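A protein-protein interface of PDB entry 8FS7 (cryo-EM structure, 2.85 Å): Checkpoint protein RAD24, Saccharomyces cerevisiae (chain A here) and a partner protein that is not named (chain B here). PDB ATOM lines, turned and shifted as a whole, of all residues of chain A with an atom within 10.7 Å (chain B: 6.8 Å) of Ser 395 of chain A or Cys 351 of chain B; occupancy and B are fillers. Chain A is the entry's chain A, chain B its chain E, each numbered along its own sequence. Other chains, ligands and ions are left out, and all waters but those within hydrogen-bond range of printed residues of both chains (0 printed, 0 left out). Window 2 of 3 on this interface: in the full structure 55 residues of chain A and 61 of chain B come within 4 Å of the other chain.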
ATOM      1  N   TYR A 384      11.027 -24.890  14.430  1.00  0.00           N
ATOM      2  CA  TYR A 384      10.750 -24.644  13.019  1.00  0.00           C
ATOM      3  C   TYR A 384      10.579 -25.929  12.218  1.00  0.00           C
ATOM      4  O   TYR A 384      10.056 -25.879  11.099  1.00  0.00           O
ATOM      5  CB  TYR A 384      11.860 -23.784  12.410  1.00  0.00           C
ATOM      6  CG  TYR A 384      13.022 -24.573  11.856  1.00  0.00           C
ATOM      7  CD1 TYR A 384      13.940 -25.178  12.703  1.00  0.00           C
ATOM      8  CD2 TYR A 384      13.209 -24.704  10.487  1.00  0.00           C
ATOM      9  CE1 TYR A 384      15.006 -25.898  12.203  1.00  0.00           C
ATOM     10  CE2 TYR A 384      14.270 -25.422   9.978  1.00  0.00           C
ATOM     11  CZ  TYR A 384      15.167 -26.017  10.840  1.00  0.00           C
ATOM     12  OH  TYR A 384      16.227 -26.733  10.336  1.00  0.00           O
ATOM     13  N   GLY A 390       8.360 -31.946   9.746  1.00  0.00           N
ATOM     14  CA  GLY A 390       9.624 -32.046   9.048  1.00  0.00           C
ATOM     15  C   GLY A 390       9.524 -32.315   7.564  1.00  0.00           C
ATOM     16  O   GLY A 390      10.544 -32.627   6.940  1.00  0.00           O
ATOM     17  N   GLU A 391       8.333 -32.210   6.978  1.00  0.00           N
ATOM     18  CA  GLU A 391       8.145 -32.498   5.557  1.00  0.00           C
ATOM     19  C   GLU A 391       8.130 -31.196   4.756  1.00  0.00           C
ATOM     20  O   GLU A 391       7.090 -30.688   4.336  1.00  0.00           O
ATOM     21  CB  GLU A 391       6.865 -33.302   5.345  1.00  0.00           C
ATOM     22  CG  GLU A 391       7.023 -34.479   4.399  1.00  0.00           C
ATOM     23  CD  GLU A 391       7.857 -35.596   4.993  1.00  0.00           C
ATOM     24  OE1 GLU A 391       7.828 -35.769   6.230  1.00  0.00           O
ATOM     25  OE2 GLU A 391       8.543 -36.302   4.224  1.00  0.00           O
ATOM     26  N   PHE A 392       9.331 -30.659   4.549  1.00  0.00           N
ATOM     27  CA  PHE A 392       9.516 -29.509   3.677  1.00  0.00           C
ATOM     28  C   PHE A 392      10.936 -29.541   3.129  1.00  0.00           C
ATOM     29  O   PHE A 392      11.790 -30.297   3.600  1.00  0.00           O
ATOM     30  CB  PHE A 392       9.222 -28.182   4.393  1.00  0.00           C
ATOM     31  CG  PHE A 392       9.910 -28.029   5.722  1.00  0.00           C
ATOM     32  CD1 PHE A 392       9.317 -28.493   6.885  1.00  0.00           C
ATOM     33  CD2 PHE A 392      11.140 -27.398   5.808  1.00  0.00           C
ATOM     34  CE1 PHE A 392       9.944 -28.344   8.107  1.00  0.00           C
ATOM     35  CE2 PHE A 392      11.772 -27.247   7.028  1.00  0.00           C
ATOM     36  CZ  PHE A 392      11.173 -27.720   8.178  1.00  0.00           C
ATOM     37  N   SER A 393      11.173 -28.715   2.112  1.00  0.00           N
ATOM     38  CA  SER A 393      12.449 -28.721   1.409  1.00  0.00           C
ATOM     39  C   SER A 393      13.591 -28.316   2.335  1.00  0.00           C
ATOM     40  O   SER A 393      13.434 -27.473   3.223  1.00  0.00           O
ATOM     41  CB  SER A 393      12.395 -27.782   0.204  1.00  0.00           C
ATOM     42  OG  SER A 393      13.673 -27.645  -0.393  1.00  0.00           O
ATOM     43  N   ILE A 394      14.753 -28.936   2.118  1.00  0.00           N
ATOM     44  CA  ILE A 394      15.929 -28.636   2.926  1.00  0.00           C
ATOM     45  C   ILE A 394      16.458 -27.234   2.649  1.00  0.00           C
ATOM     46  O   ILE A 394      17.163 -26.665   3.491  1.00  0.00           O
ATOM     47  CB  ILE A 394      17.016 -29.705   2.690  1.00  0.00           C
ATOM     48  CG1 ILE A 394      18.076 -29.662   3.795  1.00  0.00           C
ATOM     49  CG2 ILE A 394      17.656 -29.540   1.317  1.00  0.00           C
ATOM     50  CD1 ILE A 394      17.527 -29.927   5.178  1.00  0.00           C
ATOM     51  N   SER A 395      16.127 -26.652   1.493  1.00  0.00           N
ATOM     52  CA  SER A 395      16.558 -25.289   1.198  1.00  0.00           C
ATOM     53  C   SER A 395      15.927 -24.290   2.159  1.00  0.00           C
ATOM     54  O   SER A 395      16.592 -23.355   2.621  1.00  0.00           O
ATOM     55  CB  SER A 395      16.215 -24.932  -0.249  1.00  0.00           C
ATOM     56  OG  SER A 395      16.845 -25.819  -1.156  1.00  0.00           O
ATOM     57  N   ASP A 396      14.641 -24.474   2.475  1.00  0.00           N
ATOM     58  CA  ASP A 396      13.971 -23.583   3.416  1.00  0.00           C
ATOM     59  C   ASP A 396      14.583 -23.685   4.809  1.00  0.00           C
ATOM     60  O   ASP A 396      14.811 -22.665   5.474  1.00  0.00           O
ATOM     61  CB  ASP A 396      12.477 -23.903   3.460  1.00  0.00           C
ATOM     62  N   ALA A 397      14.859 -24.911   5.264  1.00  0.00           N
ATOM     63  CA  ALA A 397      15.488 -25.096   6.567  1.00  0.00           C
ATOM     64  C   ALA A 397      16.879 -24.478   6.600  1.00  0.00           C
ATOM     65  O   ALA A 397      17.262 -23.842   7.591  1.00  0.00           O
ATOM     66  CB  ALA A 397      15.555 -26.585   6.908  1.00  0.00           C
ATOM     67  N   SER A 398      17.647 -24.657   5.521  1.00  0.00           N
ATOM     68  CA  SER A 398      18.979 -24.067   5.445  1.00  0.00           C
ATOM     69  C   SER A 398      18.909 -22.547   5.481  1.00  0.00           C
ATOM     70  O   SER A 398      19.715 -21.900   6.156  1.00  0.00           O
ATOM     71  CB  SER A 398      19.694 -24.542   4.181  1.00  0.00           C
ATOM     72  OG  SER A 398      19.118 -23.965   3.023  1.00  0.00           O
ATOM     73  N   SER A 399      17.945 -21.961   4.766  1.00  0.00           N
ATOM     74  CA  SER A 399      17.778 -20.512   4.796  1.00  0.00           C
ATOM     75  C   SER A 399      17.418 -20.024   6.193  1.00  0.00           C
ATOM     76  O   SER A 399      17.953 -19.013   6.664  1.00  0.00           O
ATOM     77  CB  SER A 399      16.713 -20.085   3.786  1.00  0.00           C
ATOM     78  OG  SER A 399      17.014 -20.573   2.490  1.00  0.00           O
ATOM     79  N   ILE A 400      16.519 -20.740   6.877  1.00  0.00           N
ATOM     80  CA  ILE A 400      16.103 -20.332   8.218  1.00  0.00           C
ATOM     81  C   ILE A 400      17.281 -20.377   9.185  1.00  0.00           C
ATOM     82  O   ILE A 400      17.524 -19.429   9.945  1.00  0.00           O
ATOM     83  CB  ILE A 400      14.936 -21.208   8.708  1.00  0.00           C
ATOM     84  CG1 ILE A 400      13.659 -20.888   7.929  1.00  0.00           C
ATOM     85  CG2 ILE A 400      14.710 -21.017  10.202  1.00  0.00           C
ATOM     86  CD1 ILE A 400      12.474 -21.740   8.326  1.00  0.00           C
ATOM     87  N   VAL A 401      18.042 -21.475   9.165  1.00  0.00           N
ATOM     88  CA  VAL A 401      19.143 -21.606  10.117  1.00  0.00           C
ATOM     89  C   VAL A 401      20.278 -20.646   9.770  1.00  0.00           C
ATOM     90  O   VAL A 401      20.957 -20.126  10.663  1.00  0.00           O
ATOM     91  CB  VAL A 401      19.624 -23.067  10.204  1.00  0.00           C
ATOM     92  CG1 VAL A 401      18.500 -23.964  10.700  1.00  0.00           C
ATOM     93  CG2 VAL A 401      20.142 -23.551   8.872  1.00  0.00           C
ATOM     94  N   ASP A 402      20.496 -20.379   8.477  1.00  0.00           N
ATOM     95  CA  ASP A 402      21.501 -19.397   8.084  1.00  0.00           C
ATOM     96  C   ASP A 402      21.111 -17.999   8.546  1.00  0.00           C
ATOM     97  O   ASP A 402      21.959 -17.238   9.026  1.00  0.00           O
ATOM     98  CB  ASP A 402      21.695 -19.427   6.568  1.00  0.00           C
ATOM     99  CG  ASP A 402      22.905 -18.635   6.119  1.00  0.00           C
ATOM    100  OD1 ASP A 402      23.753 -18.305   6.974  1.00  0.00           O
ATOM    101  OD2 ASP A 402      23.009 -18.340   4.910  1.00  0.00           O
ATOM    102  N   CYS A 403      19.829 -17.647   8.416  1.00  0.00           N
ATOM    103  CA  CYS A 403      19.364 -16.357   8.907  1.00  0.00           C
ATOM    104  C   CYS A 403      19.515 -16.256  10.419  1.00  0.00           C
ATOM    105  O   CYS A 403      19.907 -15.208  10.941  1.00  0.00           O
ATOM    106  CB  CYS A 403      17.910 -16.135   8.497  1.00  0.00           C
ATOM    107  SG  CYS A 403      17.086 -14.821   9.412  1.00  0.00           S
ATOM    108  N   GLU A 423      12.209 -13.221   8.175  1.00  0.00           N
ATOM    109  CA  GLU A 423      12.672 -14.271   7.274  1.00  0.00           C
ATOM    110  C   GLU A 423      11.991 -15.600   7.573  1.00  0.00           C
ATOM    111  O   GLU A 423      11.592 -16.315   6.647  1.00  0.00           O
ATOM    112  CB  GLU A 423      14.191 -14.411   7.367  1.00  0.00           C
ATOM    113  CG  GLU A 423      14.741 -15.673   6.719  1.00  0.00           C
ATOM    114  CD  GLU A 423      14.976 -15.512   5.230  1.00  0.00           C
ATOM    115  OE1 GLU A 423      15.386 -14.412   4.807  1.00  0.00           O
ATOM    116  OE2 GLU A 423      14.752 -16.487   4.483  1.00  0.00           O
ATOM    117  N   VAL A 424      11.837 -15.942   8.855  1.00  0.00           N
ATOM    118  CA  VAL A 424      11.162 -17.191   9.210  1.00  0.00           C
ATOM    119  C   VAL A 424       9.714 -17.165   8.735  1.00  0.00           C
ATOM    120  O   VAL A 424       9.211 -18.137   8.152  1.00  0.00           O
ATOM    121  CB  VAL A 424      11.259 -17.441  10.726  1.00  0.00           C
ATOM    122  CG1 VAL A 424      10.285 -18.530  11.154  1.00  0.00           C
ATOM    123  CG2 VAL A 424      12.681 -17.820  11.110  1.00  0.00           C
ATOM    124  N   LYS A 426       8.371 -15.317   6.303  1.00  0.00           N
ATOM    125  CA  LYS A 426       8.313 -15.361   4.844  1.00  0.00           C
ATOM    126  C   LYS A 426       8.582 -16.766   4.323  1.00  0.00           C
ATOM    127  O   LYS A 426       7.898 -17.240   3.405  1.00  0.00           O
ATOM    128  CB  LYS A 426       9.314 -14.366   4.252  1.00  0.00           C
ATOM    129  CG  LYS A 426       9.333 -14.316   2.730  1.00  0.00           C
ATOM    130  CD  LYS A 426      10.550 -15.029   2.153  1.00  0.00           C
ATOM    131  CE  LYS A 426      11.843 -14.504   2.755  1.00  0.00           C
ATOM    132  NZ  LYS A 426      13.035 -15.216   2.217  1.00  0.00           N
ATOM    133  N   THR A 427       9.575 -17.450   4.901  1.00  0.00           N
ATOM    134  CA  THR A 427       9.897 -18.805   4.475  1.00  0.00           C
ATOM    135  C   THR A 427       8.728 -19.750   4.716  1.00  0.00           C
ATOM    136  O   THR A 427       8.393 -20.568   3.852  1.00  0.00           O
ATOM    137  CB  THR A 427      11.147 -19.296   5.207  1.00  0.00           C
ATOM    138  OG1 THR A 427      12.268 -18.481   4.843  1.00  0.00           O
ATOM    139  CG2 THR A 427      11.446 -20.741   4.854  1.00  0.00           C
ATOM    140  N   PHE A 428       8.081 -19.642   5.877  1.00  0.00           N
ATOM    141  CA  PHE A 428       6.951 -20.515   6.166  1.00  0.00           C
ATOM    142  C   PHE A 428       5.687 -20.117   5.412  1.00  0.00           C
ATOM    143  O   PHE A 428       4.810 -20.964   5.212  1.00  0.00           O
ATOM    144  CB  PHE A 428       6.688 -20.541   7.670  1.00  0.00           C
ATOM    145  CG  PHE A 428       7.608 -21.456   8.422  1.00  0.00           C
ATOM    146  CD1 PHE A 428       8.110 -22.598   7.820  1.00  0.00           C
ATOM    147  CD2 PHE A 428       7.989 -21.167   9.721  1.00  0.00           C
ATOM    148  CE1 PHE A 428       8.964 -23.441   8.504  1.00  0.00           C
ATOM    149  CE2 PHE A 428       8.844 -22.006  10.409  1.00  0.00           C
ATOM    150  CZ  PHE A 428       9.331 -23.144   9.799  1.00  0.00           C
ATOM    151  N   ASN A 430       5.756 -18.848   2.196  1.00  0.00           N
ATOM    152  CA  ASN A 430       5.938 -19.227   0.798  1.00  0.00           C
ATOM    153  C   ASN A 430       5.615 -20.700   0.570  1.00  0.00           C
ATOM    154  O   ASN A 430       5.050 -21.066  -0.467  1.00  0.00           O
ATOM    155  CB  ASN A 430       7.366 -18.915   0.353  1.00  0.00           C
ATOM    156  CG  ASN A 430       7.518 -17.501  -0.170  1.00  0.00           C
ATOM    157  OD1 ASN A 430       6.539 -16.765  -0.298  1.00  0.00           O
ATOM    158  ND2 ASN A 430       8.750 -17.111  -0.474  1.00  0.00           N
ATOM    159  N   ILE A 431       5.967 -21.563   1.530  1.00  0.00           N
ATOM    160  CA  ILE A 431       5.741 -22.999   1.393  1.00  0.00           C
ATOM    161  C   ILE A 431       4.419 -23.454   1.999  1.00  0.00           C
ATOM    162  O   ILE A 431       4.087 -24.645   1.910  1.00  0.00           O
ATOM    163  CB  ILE A 431       6.920 -23.780   2.015  1.00  0.00           C
ATOM    164  CG1 ILE A 431       6.679 -24.040   3.506  1.00  0.00           C
ATOM    165  CG2 ILE A 431       8.230 -23.044   1.788  1.00  0.00           C
ATOM    166  CD1 ILE A 431       7.762 -24.857   4.164  1.00  0.00           C
ATOM    167  N   ARG B 274      19.695 -36.769   3.845  1.00  0.00           N
ATOM    168  CA  ARG B 274      19.672 -35.309   3.767  1.00  0.00           C
ATOM    169  C   ARG B 274      18.211 -34.866   3.824  1.00  0.00           C
ATOM    170  O   ARG B 274      17.551 -34.734   2.791  1.00  0.00           O
ATOM    171  CB  ARG B 274      20.361 -34.809   2.494  1.00  0.00           C
ATOM    172  CG  ARG B 274      21.776 -35.329   2.301  1.00  0.00           C
ATOM    173  CD  ARG B 274      22.283 -35.037   0.899  1.00  0.00           C
ATOM    174  NE  ARG B 274      21.654 -35.894  -0.100  1.00  0.00           N
ATOM    175  CZ  ARG B 274      22.054 -37.124  -0.392  1.00  0.00           C
ATOM    176  NH1 ARG B 274      23.085 -37.680   0.223  1.00  0.00           N
ATOM    177  NH2 ARG B 274      21.403 -37.815  -1.323  1.00  0.00           N
ATOM    178  N   TYR B 324      31.716 -23.251   3.238  1.00  0.00           N
ATOM    179  CA  TYR B 324      30.734 -23.128   4.309  1.00  0.00           C
ATOM    180  C   TYR B 324      31.394 -23.269   5.672  1.00  0.00           C
ATOM    181  O   TYR B 324      31.001 -22.598   6.632  1.00  0.00           O
ATOM    182  CB  TYR B 324      29.625 -24.168   4.141  1.00  0.00           C
ATOM    183  CG  TYR B 324      28.849 -24.055   2.847  1.00  0.00           C
ATOM    184  CD1 TYR B 324      28.713 -22.833   2.198  1.00  0.00           C
ATOM    185  CD2 TYR B 324      28.244 -25.169   2.280  1.00  0.00           C
ATOM    186  CE1 TYR B 324      28.003 -22.728   1.016  1.00  0.00           C
ATOM    187  CE2 TYR B 324      27.532 -25.072   1.099  1.00  0.00           C
ATOM    188  CZ  TYR B 324      27.415 -23.850   0.472  1.00  0.00           C
ATOM    189  OH  TYR B 324      26.707 -23.750  -0.703  1.00  0.00           O
ATOM    190  N   ILE B 346      25.655 -27.628   9.004  1.00  0.00           N
ATOM    191  CA  ILE B 346      25.160 -28.950   8.625  1.00  0.00           C
ATOM    192  C   ILE B 346      24.060 -28.830   7.575  1.00  0.00           C
ATOM    193  O   ILE B 346      24.023 -29.598   6.604  1.00  0.00           O
ATOM    194  CB  ILE B 346      24.687 -29.726   9.868  1.00  0.00           C
ATOM    195  CG1 ILE B 346      25.887 -30.094  10.745  1.00  0.00           C
ATOM    196  CG2 ILE B 346      23.927 -30.980   9.462  1.00  0.00           C
ATOM    197  CD1 ILE B 346      25.610 -31.201  11.742  1.00  0.00           C
ATOM    198  N   ALA B 347      23.157 -27.861   7.743  1.00  0.00           N
ATOM    199  CA  ALA B 347      22.090 -27.667   6.764  1.00  0.00           C
ATOM    200  C   ALA B 347      22.641 -27.225   5.414  1.00  0.00           C
ATOM    201  O   ALA B 347      22.138 -27.649   4.368  1.00  0.00           O
ATOM    202  CB  ALA B 347      21.074 -26.656   7.288  1.00  0.00           C
ATOM    203  N   LYS B 348      23.664 -26.366   5.413  1.00  0.00           N
ATOM    204  CA  LYS B 348      24.286 -25.954   4.157  1.00  0.00           C
ATOM    205  C   LYS B 348      24.960 -27.133   3.466  1.00  0.00           C
ATOM    206  O   LYS B 348      24.873 -27.274   2.240  1.00  0.00           O
ATOM    207  CB  LYS B 348      25.293 -24.833   4.412  1.00  0.00           C
ATOM    208  CG  LYS B 348      24.663 -23.467   4.631  1.00  0.00           C
ATOM    209  CD  LYS B 348      24.174 -22.866   3.323  1.00  0.00           C
ATOM    210  CE  LYS B 348      23.659 -21.452   3.527  1.00  0.00           C
ATOM    211  NZ  LYS B 348      23.211 -20.834   2.249  1.00  0.00           N
ATOM    212  N   VAL B 349      25.630 -27.993   4.236  1.00  0.00           N
ATOM    213  CA  VAL B 349      26.237 -29.189   3.657  1.00  0.00           C
ATOM    214  C   VAL B 349      25.166 -30.092   3.058  1.00  0.00           C
ATOM    215  O   VAL B 349      25.327 -30.624   1.952  1.00  0.00           O
ATOM    216  CB  VAL B 349      27.081 -29.925   4.716  1.00  0.00           C
ATOM    217  CG1 VAL B 349      27.441 -31.325   4.241  1.00  0.00           C
ATOM    218  CG2 VAL B 349      28.339 -29.133   5.030  1.00  0.00           C
ATOM    219  N   MET B 350      24.051 -30.270   3.773  1.00  0.00           N
ATOM    220  CA  MET B 350      22.964 -31.103   3.265  1.00  0.00           C
ATOM    221  C   MET B 350      22.364 -30.522   1.990  1.00  0.00           C
ATOM    222  O   MET B 350      22.063 -31.259   1.043  1.00  0.00           O
ATOM    223  CB  MET B 350      21.887 -31.264   4.337  1.00  0.00           C
ATOM    224  CG  MET B 350      22.295 -32.157   5.494  1.00  0.00           C
ATOM    225  SD  MET B 350      20.909 -32.599   6.557  1.00  0.00           S
ATOM    226  CE  MET B 350      21.520 -34.114   7.288  1.00  0.00           C
ATOM    227  N   CYS B 351      22.182 -29.200   1.946  1.00  0.00           N
ATOM    228  CA  CYS B 351      21.619 -28.553   0.767  1.00  0.00           C
ATOM    229  C   CYS B 351      22.608 -28.500  -0.391  1.00  0.00           C
ATOM    230  O   CYS B 351      22.192 -28.295  -1.536  1.00  0.00           O
ATOM    231  CB  CYS B 351      21.149 -27.140   1.123  1.00  0.00           C
ATOM    232  SG  CYS B 351      20.145 -26.325  -0.141  1.00  0.00           S
ATOM    233  N   CYS B 352      23.903 -28.661  -0.120  1.00  0.00           N
ATOM    234  CA  CYS B 352      24.877 -28.710  -1.205  1.00  0.00           C
ATOM    235  C   CYS B 352      25.045 -30.125  -1.748  1.00  0.00           C
ATOM    236  O   CYS B 352      25.279 -30.307  -2.948  1.00  0.00           O
ATOM    237  CB  CYS B 352      26.221 -28.159  -0.730  1.00  0.00           C
ATOM    238  SG  CYS B 352      27.431 -29.422  -0.276  1.00  0.00           S
ATOM    239  N   LEU B 353      24.929 -31.138  -0.884  1.00  0.00           N
ATOM    240  CA  LEU B 353      25.174 -32.510  -1.320  1.00  0.00           C
ATOM    241  C   LEU B 353      24.013 -33.078  -2.131  1.00  0.00           C
ATOM    242  O   LEU B 353      24.230 -33.939  -2.990  1.00  0.00           O
ATOM    243  CB  LEU B 353      25.455 -33.407  -0.114  1.00  0.00           C
ATOM    244  CG  LEU B 353      26.772 -33.181   0.631  1.00  0.00           C
ATOM    245  CD1 LEU B 353      26.928 -34.185   1.762  1.00  0.00           C
ATOM    246  CD2 LEU B 353      27.953 -33.257  -0.323  1.00  0.00           C
ATOM    247  N   ASP B 354      22.790 -32.623  -1.877  1.00  0.00           N
ATOM    248  CA  ASP B 354      21.615 -33.206  -2.525  1.00  0.00           C
ATOM    249  C   ASP B 354      21.564 -32.903  -4.022  1.00  0.00           C
ATOM    250  O   ASP B 354      20.802 -33.521  -4.766  1.00  0.00           O
ATOM    251  CB  ASP B 354      20.329 -32.720  -1.842  1.00  0.00           C
ATOM    252  CG  ASP B 354      19.960 -31.293  -2.215  1.00  0.00           C
ATOM    253  OD1 ASP B 354      20.865 -30.492  -2.526  1.00  0.00           O
ATOM    254  OD2 ASP B 354      18.753 -30.971  -2.197  1.00  0.00           O
ATOM    255  OXT ASP B 354      22.280 -32.036  -4.524  1.00  0.00           O
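Of the printed residues of chain B, Ile 394 of chain A touches Asp 354 (3.9 Å).
Ser 395 of chain A touches just one residue of chain B: Cys 351 (3.5 Å).
Printed residues of chain B within 4 Å of Val 401 of chain A: Ala 347 (3.6 Å).
Of the printed residues of chain B, Asp 402 of chain A touches Lys 348.
Of the printed residues of chain A, Lys 348 of chain B touches Asp 402.
Cys 351 of chain B touches just one residue of chain A: Ser 395.
No residue of chain A comes within 4 Å of Cys 352 of chain B.
Of the printed residues of chain A, Asp 354 of chain B touches Ile 394 (3.9 Å).
Ile 394 of chain A touches Asp 354 of chain B (CG2 to OD2, 3.9 Å).
CA of Ser 398 of chain A touches CB of Ala 347 of chain B, 3.8 Å away.
Val 401 of chain A touches Ala 347 of chain B.
The backbone carbonyl oxygen (O) of Ser 395 of chain A lies within hydrogen-bond range of the side-chain hydroxyl (OG) of Ser 398 of chain A (2.6 Å).
OG of Ser 399 of chain A is in hydrogen-bond range of O of Ser 395 of chain A.
The backbone carbonyl oxygen (O) of Ile 394 of chain A is in hydrogen-bond range of the side-chain hydroxyl (OG) of Ser 398 of chain A (3.4 Å).
N of Ser 395 of chain A lies close to OG of Ser 393 of chain A (3.3 Å).
OD2 of Asp 402 of chain A lies within salt-bridge range of NZ of Lys 348 of chain B.
OG of Ser 395 of chain A is in hydrogen-bond range of SG of Cys 351 of chain B, at 3.5 Å.
Of the 22 printed residues of chain A, 5 touch a printed residue of chain B.
Printed residues of chain A that touch a printed residue of chain B: Ile 394, Ser 395, Ser 398, Val 401 and Asp 402.
Hydrophobic or aromatic side chains of chain A within 4 Å of the printed part of chain B: Ile 394 and Val 401.
Of the 11 printed residues of chain B, 4 touch a printed residue of chain A.
Hydrophobic or aromatic side chains of chain B that line the printed part of chain A: Ala 347.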
